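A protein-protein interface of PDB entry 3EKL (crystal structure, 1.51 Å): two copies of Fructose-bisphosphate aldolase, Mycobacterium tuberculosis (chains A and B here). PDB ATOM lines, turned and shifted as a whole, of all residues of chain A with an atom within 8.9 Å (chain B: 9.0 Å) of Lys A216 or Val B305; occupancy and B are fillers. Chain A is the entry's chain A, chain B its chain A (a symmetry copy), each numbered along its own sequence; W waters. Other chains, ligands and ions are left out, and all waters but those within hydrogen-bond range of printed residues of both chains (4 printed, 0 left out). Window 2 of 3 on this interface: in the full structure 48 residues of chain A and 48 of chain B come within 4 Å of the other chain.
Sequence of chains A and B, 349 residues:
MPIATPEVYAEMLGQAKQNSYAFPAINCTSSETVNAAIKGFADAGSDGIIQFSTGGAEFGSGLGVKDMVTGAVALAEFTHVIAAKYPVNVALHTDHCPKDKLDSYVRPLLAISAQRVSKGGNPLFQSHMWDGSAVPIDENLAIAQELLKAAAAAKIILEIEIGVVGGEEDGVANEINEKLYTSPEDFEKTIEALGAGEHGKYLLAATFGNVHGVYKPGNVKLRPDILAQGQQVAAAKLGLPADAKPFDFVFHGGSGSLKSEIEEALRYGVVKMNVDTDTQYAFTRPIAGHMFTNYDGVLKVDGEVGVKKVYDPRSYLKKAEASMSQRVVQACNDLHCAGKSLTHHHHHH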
ATOM      1  N   GLY A 213     -22.815 -30.190  12.556  1.00  0.00           N
ATOM      2  CA  GLY A 213     -22.437 -29.133  11.607  1.00  0.00           C
ATOM      3  C   GLY A 213     -22.276 -29.624  10.176  1.00  0.00           C
ATOM      4  O   GLY A 213     -22.461 -30.814   9.898  1.00  0.00           O
ATOM      5  N   VAL A 214     -21.942 -28.713   9.265  1.00  0.00           N
ATOM      6  CA  VAL A 214     -21.728 -29.067   7.862  1.00  0.00           C
ATOM      7  C   VAL A 214     -20.395 -28.515   7.372  1.00  0.00           C
ATOM      8  O   VAL A 214     -20.170 -27.300   7.388  1.00  0.00           O
ATOM      9  CB  VAL A 214     -22.890 -28.590   6.943  1.00  0.00           C
ATOM     10  CG1 VAL A 214     -22.505 -28.678   5.474  1.00  0.00           C
ATOM     11  CG2 VAL A 214     -24.118 -29.433   7.179  1.00  0.00           C
ATOM     12  N   TYR A 215     -19.534 -29.426   6.927  1.00  0.00           N
ATOM     13  CA  TYR A 215     -18.189 -29.097   6.467  1.00  0.00           C
ATOM     14  C   TYR A 215     -17.974 -29.627   5.049  1.00  0.00           C
ATOM     15  O   TYR A 215     -18.803 -30.379   4.528  1.00  0.00           O
ATOM     16  CB  TYR A 215     -17.147 -29.711   7.413  1.00  0.00           C
ATOM     17  CG  TYR A 215     -17.410 -29.457   8.884  1.00  0.00           C
ATOM     18  CD1 TYR A 215     -18.294 -30.264   9.605  1.00  0.00           C
ATOM     19  CD2 TYR A 215     -16.775 -28.414   9.557  1.00  0.00           C
ATOM     20  CE1 TYR A 215     -18.545 -30.032  10.949  1.00  0.00           C
ATOM     21  CE2 TYR A 215     -17.017 -28.176  10.908  1.00  0.00           C
ATOM     22  CZ  TYR A 215     -17.902 -28.992  11.597  1.00  0.00           C
ATOM     23  OH  TYR A 215     -18.147 -28.766  12.932  1.00  0.00           O
ATOM     24  N   LYS A 216     -16.866 -29.224   4.430  1.00  0.00           N
ATOM     25  CA  LYS A 216     -16.448 -29.763   3.137  1.00  0.00           C
ATOM     26  C   LYS A 216     -16.026 -31.237   3.277  1.00  0.00           C
ATOM     27  O   LYS A 216     -15.634 -31.664   4.369  1.00  0.00           O
ATOM     28  CB  LYS A 216     -15.303 -28.924   2.562  1.00  0.00           C
ATOM     29  CG  LYS A 216     -15.702 -27.510   2.161  1.00  0.00           C
ATOM     30  CD  LYS A 216     -14.504 -26.720   1.663  1.00  0.00           C
ATOM     31  CE  LYS A 216     -14.889 -25.293   1.312  1.00  0.00           C
ATOM     32  NZ  LYS A 216     -13.714 -24.503   0.858  1.00  0.00           N
ATOM     33  N   PRO A 217     -16.113 -32.022   2.178  1.00  0.00           N
ATOM     34  CA  PRO A 217     -15.736 -33.444   2.215  1.00  0.00           C
ATOM     35  C   PRO A 217     -14.269 -33.666   2.587  1.00  0.00           C
ATOM     36  O   PRO A 217     -13.406 -32.865   2.218  1.00  0.00           O
ATOM     37  CB  PRO A 217     -15.981 -33.914   0.775  1.00  0.00           C
ATOM     38  CG  PRO A 217     -16.925 -32.925   0.195  1.00  0.00           C
ATOM     39  CD  PRO A 217     -16.582 -31.621   0.837  1.00  0.00           C
ATOM     40  N   GLY A 218     -14.001 -34.749   3.312  1.00  0.00           N
ATOM     41  CA  GLY A 218     -12.644 -35.081   3.749  1.00  0.00           C
ATOM     42  C   GLY A 218     -12.364 -34.688   5.190  1.00  0.00           C
ATOM     43  O   GLY A 218     -11.408 -35.178   5.799  1.00  0.00           O
ATOM     44  N   ASN A 219     -13.197 -33.798   5.729  1.00  0.00           N
ATOM     45  CA  ASN A 219     -13.078 -33.344   7.113  1.00  0.00           C
ATOM     46  C   ASN A 219     -13.631 -34.386   8.082  1.00  0.00           C
ATOM     47  O   ASN A 219     -12.878 -34.980   8.863  1.00  0.00           O
ATOM     48  CB  ASN A 219     -13.791 -31.997   7.305  1.00  0.00           C
ATOM     49  CG  ASN A 219     -13.049 -30.836   6.657  1.00  0.00           C
ATOM     50  OD1 ASN A 219     -12.765 -29.832   7.311  1.00  0.00           O
ATOM     51  ND2 ASN A 219     -12.739 -30.965   5.370  1.00  0.00           N
ATOM     52  N   VAL A 220     -14.945 -34.597   8.014  1.00  0.00           N
ATOM     53  CA  VAL A 220     -15.630 -35.582   8.847  1.00  0.00           C
ATOM     54  C   VAL A 220     -15.264 -37.001   8.407  1.00  0.00           C
ATOM     55  O   VAL A 220     -15.372 -37.337   7.222  1.00  0.00           O
ATOM     56  CB  VAL A 220     -17.168 -35.368   8.832  1.00  0.00           C
ATOM     57  CG1 VAL A 220     -17.554 -34.229   9.761  1.00  0.00           C
ATOM     58  CG2 VAL A 220     -17.672 -35.085   7.418  1.00  0.00           C
ATOM     59  N   LYS A 221     -14.819 -37.820   9.357  1.00  0.00           N
ATOM     60  CA  LYS A 221     -14.358 -39.175   9.058  1.00  0.00           C
ATOM     61  C   LYS A 221     -15.161 -40.223   9.832  1.00  0.00           C
ATOM     62  O   LYS A 221     -14.772 -40.646  10.925  1.00  0.00           O
ATOM     63  CB  LYS A 221     -12.857 -39.304   9.350  1.00  0.00           C
ATOM     64  CG  LYS A 221     -12.188 -40.514   8.714  1.00  0.00           C
ATOM     65  CD  LYS A 221     -10.686 -40.497   8.955  1.00  0.00           C
ATOM     66  CE  LYS A 221      -9.992 -41.631   8.220  1.00  0.00           C
ATOM     67  NZ  LYS A 221      -8.515 -41.582   8.403  1.00  0.00           N
ATOM     68  N   GLY A 256     -24.971 -33.033   5.989  1.00  0.00           N
ATOM     69  CA  GLY A 256     -23.708 -33.059   5.255  1.00  0.00           C
ATOM     70  C   GLY A 256     -23.134 -34.437   4.972  1.00  0.00           C
ATOM     71  O   GLY A 256     -22.095 -34.546   4.306  1.00  0.00           O
ATOM     72  N   LEU A 258     -22.561 -38.291   3.479  1.00  0.00           N
ATOM     73  CA  LEU A 258     -22.637 -38.953   2.184  1.00  0.00           C
ATOM     74  C   LEU A 258     -23.730 -40.014   2.203  1.00  0.00           C
ATOM     75  O   LEU A 258     -24.035 -40.574   3.261  1.00  0.00           O
ATOM     76  CB  LEU A 258     -21.299 -39.617   1.838  1.00  0.00           C
ATOM     77  CG  LEU A 258     -20.046 -38.747   1.709  1.00  0.00           C
ATOM     78  CD1 LEU A 258     -18.823 -39.637   1.493  1.00  0.00           C
ATOM     79  CD2 LEU A 258     -20.176 -37.732   0.575  1.00  0.00           C
ATOM     80  N   THR A 277     -28.508 -28.858  10.969  1.00  0.00           N
ATOM     81  CA  THR A 277     -27.845 -27.848  10.143  1.00  0.00           C
ATOM     82  C   THR A 277     -28.424 -27.772   8.730  1.00  0.00           C
ATOM     83  O   THR A 277     -28.641 -26.669   8.216  1.00  0.00           O
ATOM     84  CB  THR A 277     -26.343 -28.070  10.057  1.00  0.00           C
ATOM     85  OG1 THR A 277     -26.105 -29.375   9.544  1.00  0.00           O
ATOM     86  CG2 THR A 277     -25.719 -27.953  11.417  1.00  0.00           C
ATOM     87  N   ASP A 278     -28.676 -28.919   8.093  1.00  0.00           N
ATOM     88  CA  ASP A 278     -29.167 -28.879   6.711  1.00  0.00           C
ATOM     89  C   ASP A 278     -30.577 -28.295   6.591  1.00  0.00           C
ATOM     90  O   ASP A 278     -30.892 -27.617   5.607  1.00  0.00           O
ATOM     91  CB  ASP A 278     -29.093 -30.249   6.045  1.00  0.00           C
ATOM     92  CG  ASP A 278     -27.699 -30.559   5.494  1.00  0.00           C
ATOM     93  OD1 ASP A 278     -26.822 -29.656   5.462  1.00  0.00           O
ATOM     94  OD2 ASP A 278     -27.500 -31.713   5.083  1.00  0.00           O
ATOM     95  N   TYR A 281     -30.220 -24.462   6.949  1.00  0.00           N
ATOM     96  CA  TYR A 281     -29.850 -23.796   5.697  1.00  0.00           C
ATOM     97  C   TYR A 281     -31.059 -23.713   4.766  1.00  0.00           C
ATOM     98  O   TYR A 281     -31.287 -22.675   4.119  1.00  0.00           O
ATOM     99  CB  TYR A 281     -28.687 -24.500   4.984  1.00  0.00           C
ATOM    100  CG  TYR A 281     -28.252 -23.728   3.749  1.00  0.00           C
ATOM    101  CD1 TYR A 281     -27.491 -22.567   3.876  1.00  0.00           C
ATOM    102  CD2 TYR A 281     -28.604 -24.143   2.463  1.00  0.00           C
ATOM    103  CE1 TYR A 281     -27.094 -21.826   2.761  1.00  0.00           C
ATOM    104  CE2 TYR A 281     -28.199 -23.419   1.330  1.00  0.00           C
ATOM    105  CZ  TYR A 281     -27.450 -22.254   1.485  1.00  0.00           C
ATOM    106  OH  TYR A 281     -27.023 -21.511   0.393  1.00  0.00           O
ATOM    107  N   ASP B 296     -22.457 -13.699   2.863  1.00  0.00           N
ATOM    108  CA  ASP B 296     -21.562 -14.804   2.497  1.00  0.00           C
ATOM    109  C   ASP B 296     -21.552 -15.908   3.538  1.00  0.00           C
ATOM    110  O   ASP B 296     -20.803 -16.889   3.404  1.00  0.00           O
ATOM    111  CB  ASP B 296     -20.139 -14.323   2.166  1.00  0.00           C
ATOM    112  CG  ASP B 296     -19.537 -13.431   3.233  1.00  0.00           C
ATOM    113  OD1 ASP B 296     -20.191 -13.164   4.265  1.00  0.00           O
ATOM    114  OD2 ASP B 296     -18.385 -12.980   3.010  1.00  0.00           O
ATOM    115  N   GLY B 297     -22.410 -15.745   4.545  1.00  0.00           N
ATOM    116  CA  GLY B 297     -22.645 -16.770   5.567  1.00  0.00           C
ATOM    117  C   GLY B 297     -24.000 -17.441   5.379  1.00  0.00           C
ATOM    118  O   GLY B 297     -24.141 -18.660   5.583  1.00  0.00           O
ATOM    119  N   VAL B 298     -25.009 -16.658   5.000  1.00  0.00           N
ATOM    120  CA  VAL B 298     -26.352 -17.203   4.751  1.00  0.00           C
ATOM    121  C   VAL B 298     -26.509 -17.785   3.345  1.00  0.00           C
ATOM    122  O   VAL B 298     -27.484 -18.520   3.074  1.00  0.00           O
ATOM    123  CB  VAL B 298     -27.495 -16.177   5.063  1.00  0.00           C
ATOM    124  CG1 VAL B 298     -27.422 -15.700   6.528  1.00  0.00           C
ATOM    125  CG2 VAL B 298     -27.465 -14.995   4.098  1.00  0.00           C
ATOM    126  N   LEU B 299     -25.549 -17.468   2.461  1.00  0.00           N
ATOM    127  CA  LEU B 299     -25.448 -18.078   1.126  1.00  0.00           C
ATOM    128  C   LEU B 299     -24.158 -18.867   1.025  1.00  0.00           C
ATOM    129  O   LEU B 299     -23.125 -18.452   1.554  1.00  0.00           O
ATOM    130  CB  LEU B 299     -25.442 -17.014   0.021  1.00  0.00           C
ATOM    131  CG  LEU B 299     -26.627 -16.047  -0.034  1.00  0.00           C
ATOM    132  CD1 LEU B 299     -26.372 -15.004  -1.115  1.00  0.00           C
ATOM    133  CD2 LEU B 299     -27.950 -16.788  -0.280  1.00  0.00           C
ATOM    134  N   LYS B 300     -24.234 -20.004   0.333  1.00  0.00           N
ATOM    135  CA  LYS B 300     -23.052 -20.795  -0.008  1.00  0.00           C
ATOM    136  C   LYS B 300     -22.500 -20.195  -1.296  1.00  0.00           C
ATOM    137  O   LYS B 300     -23.064 -20.393  -2.374  1.00  0.00           O
ATOM    138  CB  LYS B 300     -23.454 -22.277  -0.155  1.00  0.00           C
ATOM    139  CG  LYS B 300     -23.941 -22.893   1.168  1.00  0.00           C
ATOM    140  CD  LYS B 300     -24.401 -24.360   1.068  1.00  0.00           C
ATOM    141  CE  LYS B 300     -24.775 -24.871   2.461  1.00  0.00           C
ATOM    142  NZ  LYS B 300     -25.211 -26.304   2.491  1.00  0.00           N
ATOM    143  N   VAL B 301     -21.425 -19.421  -1.171  1.00  0.00           N
ATOM    144  CA  VAL B 301     -20.903 -18.645  -2.301  1.00  0.00           C
ATOM    145  C   VAL B 301     -19.502 -19.098  -2.705  1.00  0.00           C
ATOM    146  O   VAL B 301     -18.697 -19.481  -1.852  1.00  0.00           O
ATOM    147  CB  VAL B 301     -20.911 -17.113  -1.999  1.00  0.00           C
ATOM    148  CG1 VAL B 301     -19.990 -16.774  -0.824  1.00  0.00           C
ATOM    149  CG2 VAL B 301     -20.574 -16.289  -3.243  1.00  0.00           C
ATOM    150  N   ASP B 302     -19.237 -19.066  -4.009  1.00  0.00           N
ATOM    151  CA  ASP B 302     -17.897 -19.336  -4.574  1.00  0.00           C
ATOM    152  C   ASP B 302     -17.301 -20.659  -4.101  1.00  0.00           C
ATOM    153  O   ASP B 302     -16.091 -20.762  -3.893  1.00  0.00           O
ATOM    154  CB  ASP B 302     -16.935 -18.170  -4.291  1.00  0.00           C
ATOM    155  CG  ASP B 302     -17.348 -16.885  -4.980  1.00  0.00           C
ATOM    156  OD1 ASP B 302     -17.646 -16.920  -6.186  1.00  0.00           O
ATOM    157  OD2 ASP B 302     -17.341 -15.838  -4.308  1.00  0.00           O
ATOM    158  N   GLY B 303     -18.174 -21.646  -3.923  1.00  0.00           N
ATOM    159  CA  GLY B 303     -17.756 -22.994  -3.511  1.00  0.00           C
ATOM    160  C   GLY B 303     -17.640 -23.195  -2.010  1.00  0.00           C
ATOM    161  O   GLY B 303     -17.326 -24.303  -1.555  1.00  0.00           O
ATOM    162  N   GLU B 304     -17.898 -22.140  -1.236  1.00  0.00           N
ATOM    163  CA  GLU B 304     -17.872 -22.237   0.229  1.00  0.00           C
ATOM    164  C   GLU B 304     -19.199 -22.796   0.748  1.00  0.00           C
ATOM    165  O   GLU B 304     -20.180 -22.889  -0.004  1.00  0.00           O
ATOM    166  CB  GLU B 304     -17.547 -20.889   0.885  1.00  0.00           C
ATOM    167  CG  GLU B 304     -16.261 -20.221   0.394  1.00  0.00           C
ATOM    168  CD  GLU B 304     -14.999 -21.016   0.697  1.00  0.00           C
ATOM    169  OE1 GLU B 304     -14.967 -21.748   1.711  1.00  0.00           O
ATOM    170  OE2 GLU B 304     -14.022 -20.896  -0.081  1.00  0.00           O
ATOM    171  N   VAL B 305     -19.222 -23.190   2.020  1.00  0.00           N
ATOM    172  CA  VAL B 305     -20.390 -23.871   2.590  1.00  0.00           C
ATOM    173  C   VAL B 305     -21.227 -23.015   3.541  1.00  0.00           C
ATOM    174  O   VAL B 305     -22.027 -23.545   4.313  1.00  0.00           O
ATOM    175  CB  VAL B 305     -20.011 -25.213   3.295  1.00  0.00           C
ATOM    176  CG1 VAL B 305     -19.482 -26.221   2.290  1.00  0.00           C
ATOM    177  CG2 VAL B 305     -19.000 -24.993   4.420  1.00  0.00           C
ATOM    178  N   GLY B 306     -21.059 -21.696   3.477  1.00  0.00           N
ATOM    179  CA  GLY B 306     -21.809 -20.799   4.361  1.00  0.00           C
ATOM    180  C   GLY B 306     -21.311 -20.903   5.795  1.00  0.00           C
ATOM    181  O   GLY B 306     -20.275 -21.542   6.062  1.00  0.00           O
ATOM    182  N   VAL B 307     -22.039 -20.259   6.709  1.00  0.00           N
ATOM    183  CA  VAL B 307     -21.643 -20.183   8.111  1.00  0.00           C
ATOM    184  C   VAL B 307     -22.860 -20.485   8.971  1.00  0.00           C
ATOM    185  O   VAL B 307     -23.781 -19.665   9.074  1.00  0.00           O
ATOM    186  CB  VAL B 307     -21.052 -18.791   8.467  1.00  0.00           C
ATOM    187  CG1 VAL B 307     -20.710 -18.699   9.953  1.00  0.00           C
ATOM    188  CG2 VAL B 307     -19.803 -18.514   7.619  1.00  0.00           C
ATOM    189  N   LYS B 308     -22.859 -21.676   9.571  1.00  0.00           N
ATOM    190  CA  LYS B 308     -24.009 -22.158  10.336  1.00  0.00           C
ATOM    191  C   LYS B 308     -24.477 -21.184  11.406  1.00  0.00           C
ATOM    192  O   LYS B 308     -25.684 -21.032  11.627  1.00  0.00           O
ATOM    193  CB  LYS B 308     -23.707 -23.529  10.949  1.00  0.00           C
ATOM    194  CG  LYS B 308     -24.751 -24.031  11.933  1.00  0.00           C
ATOM    195  CD  LYS B 308     -24.181 -25.217  12.717  1.00  0.00           C
ATOM    196  CE  LYS B 308     -25.012 -25.569  13.942  1.00  0.00           C
ATOM    197  NZ  LYS B 308     -26.374 -26.058  13.593  1.00  0.00           N
ATOM    198  N   LYS B 309     -23.540 -20.512  12.078  1.00  0.00           N
ATOM    199  CA  LYS B 309     -23.927 -19.616  13.177  1.00  0.00           C
ATOM    200  C   LYS B 309     -24.724 -18.389  12.735  1.00  0.00           C
ATOM    201  O   LYS B 309     -25.320 -17.709  13.572  1.00  0.00           O
ATOM    202  CB  LYS B 309     -22.726 -19.210  14.038  1.00  0.00           C
ATOM    203  CG  LYS B 309     -22.453 -20.176  15.181  1.00  0.00           C
ATOM    204  CD  LYS B 309     -21.574 -19.539  16.244  1.00  0.00           C
ATOM    205  CE  LYS B 309     -21.201 -20.540  17.325  1.00  0.00           C
ATOM    206  NZ  LYS B 309     -20.218 -21.553  16.842  1.00  0.00           N
ATOM    207  N   VAL B 310     -24.730 -18.104  11.432  1.00  0.00           N
ATOM    208  CA  VAL B 310     -25.577 -17.025  10.908  1.00  0.00           C
ATOM    209  C   VAL B 310     -26.742 -17.521  10.045  1.00  0.00           C
ATOM    210  O   VAL B 310     -27.672 -16.761   9.792  1.00  0.00           O
ATOM    211  CB  VAL B 310     -24.779 -15.872  10.199  1.00  0.00           C
ATOM    212  CG1 VAL B 310     -23.805 -15.208  11.177  1.00  0.00           C
ATOM    213  CG2 VAL B 310     -24.068 -16.359   8.944  1.00  0.00           C
ATOM    214  N   TYR B 311     -26.717 -18.779   9.597  1.00  0.00           N
ATOM    215  CA  TYR B 311     -27.921 -19.295   8.951  1.00  0.00           C
ATOM    216  C   TYR B 311     -28.837 -20.078   9.889  1.00  0.00           C
ATOM    217  O   TYR B 311     -29.958 -20.439   9.527  1.00  0.00           O
ATOM    218  CB  TYR B 311     -27.656 -20.001   7.610  1.00  0.00           C
ATOM    219  CG  TYR B 311     -26.885 -21.308   7.585  1.00  0.00           C
ATOM    220  CD1 TYR B 311     -27.415 -22.479   8.120  1.00  0.00           C
ATOM    221  CD2 TYR B 311     -25.667 -21.388   6.921  1.00  0.00           C
ATOM    222  CE1 TYR B 311     -26.725 -23.693   8.034  1.00  0.00           C
ATOM    223  CE2 TYR B 311     -24.963 -22.593   6.829  1.00  0.00           C
ATOM    224  CZ  TYR B 311     -25.497 -23.750   7.378  1.00  0.00           C
ATOM    225  OH  TYR B 311     -24.797 -24.945   7.271  1.00  0.00           O
HETATM  226  O   HOH W   1     -29.429 -19.982   4.292  1.00  0.00           O
HETATM  227  O   HOH W   2     -22.227 -24.816   6.625  1.00  0.00           O
HETATM  228  O   HOH W   3     -26.052 -26.841   5.172  1.00  0.00           O
HETATM  229  O   HOH W   4     -25.323 -29.714   3.174  1.00  0.00           O
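The side-chain carboxylate of Glu B304 lies within salt-bridge range of the side-chain amino group of Lys A216 (3.1 Å).
N of Lys B300 lies within hydrogen-bond range of OH of Tyr A281.
ND2 of Asn A219 lies within hydrogen-bond range of O of Lys A216 (3.1 Å).
Among the printed residues, merely in contact across the chains: Val A214 with Val B305, Lys A216 with Gly B303, Lys A216 with Val B305, Thr A277 with Lys B308, Thr A277 with Tyr B311, Tyr A281 with Val B298, Tyr A281 with Leu B299 and Tyr A281 with Tyr B311.
Printed residues of chain B within 4 Å of Lys A216: Gly B303, Glu B304 and Val B305.
Of the printed residues of chain A, Val B305 touches Val A214 (3.9 Å) and Lys A216 (3.996 Å).
No residue of chain B comes within 4 Å of Pro A217.
Glu B304 touches just one residue of chain A: Lys A216.
Of the printed residues of chain B, Tyr A281 touches Val B298, Leu B299, Lys B300 and Tyr B311.
Of the printed residues of chain A, Gly B303 touches Lys A216.
Printed residues of chain A within 4 Å of Leu B299: Tyr A281.
Of the printed residues of chain B, Thr A277 touches Lys B308 (3.0 Å) and Tyr B311 (3.5 Å).
Lys B309 touches none of the printed residues of chain A.
Asp B296 touches none of the printed residues of chain A.
The nearest printed residue of chain B that does not touch Lys A216 is Asp B302 (6.5 Å).
The nearest printed residue of chain A that does not touch Val B305 is Tyr A215 (4.6 Å).
Printed residues of chain A that touch a printed residue of chain B: Val A214, Lys A216, Thr A277 and Tyr A281.
Hydrophobic or aromatic side chains of chain A within 4 Å of the printed part of chain B: Tyr A281.
Of the 16 printed residues of chain B, 8 touch a printed residue of chain A.
Among the printed residues, Asp or Glu carboxylates within 4 Å of a Lys or Arg side-chain nitrogen of the other chain: Lys A216 with Glu B304 (3.1 Å).
No position is printed for both chains.
Water W2 lies within hydrogen-bond range of O of Val B305 (2.6 Å), OH of Tyr B311 (2.7 Å) and O of Val A214 (3.3 Å).
Water W1 bridges the backbone carbonyl oxygen of Val B298 (2.7 Å) and the backbone carbonyl oxygen of Tyr A281 (3.3 Å).
Water W4 bridges the side-chain carboxylate of Asp A278 (2.7 Å) and the side-chain amino group of Lys B300 (3.5 Å).
Water W3 lies within hydrogen-bond range of NZ of Lys B300 (2.9 Å), OD1 of Asp A278 (2.9 Å) and OH of Tyr B311 (3.1 Å).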
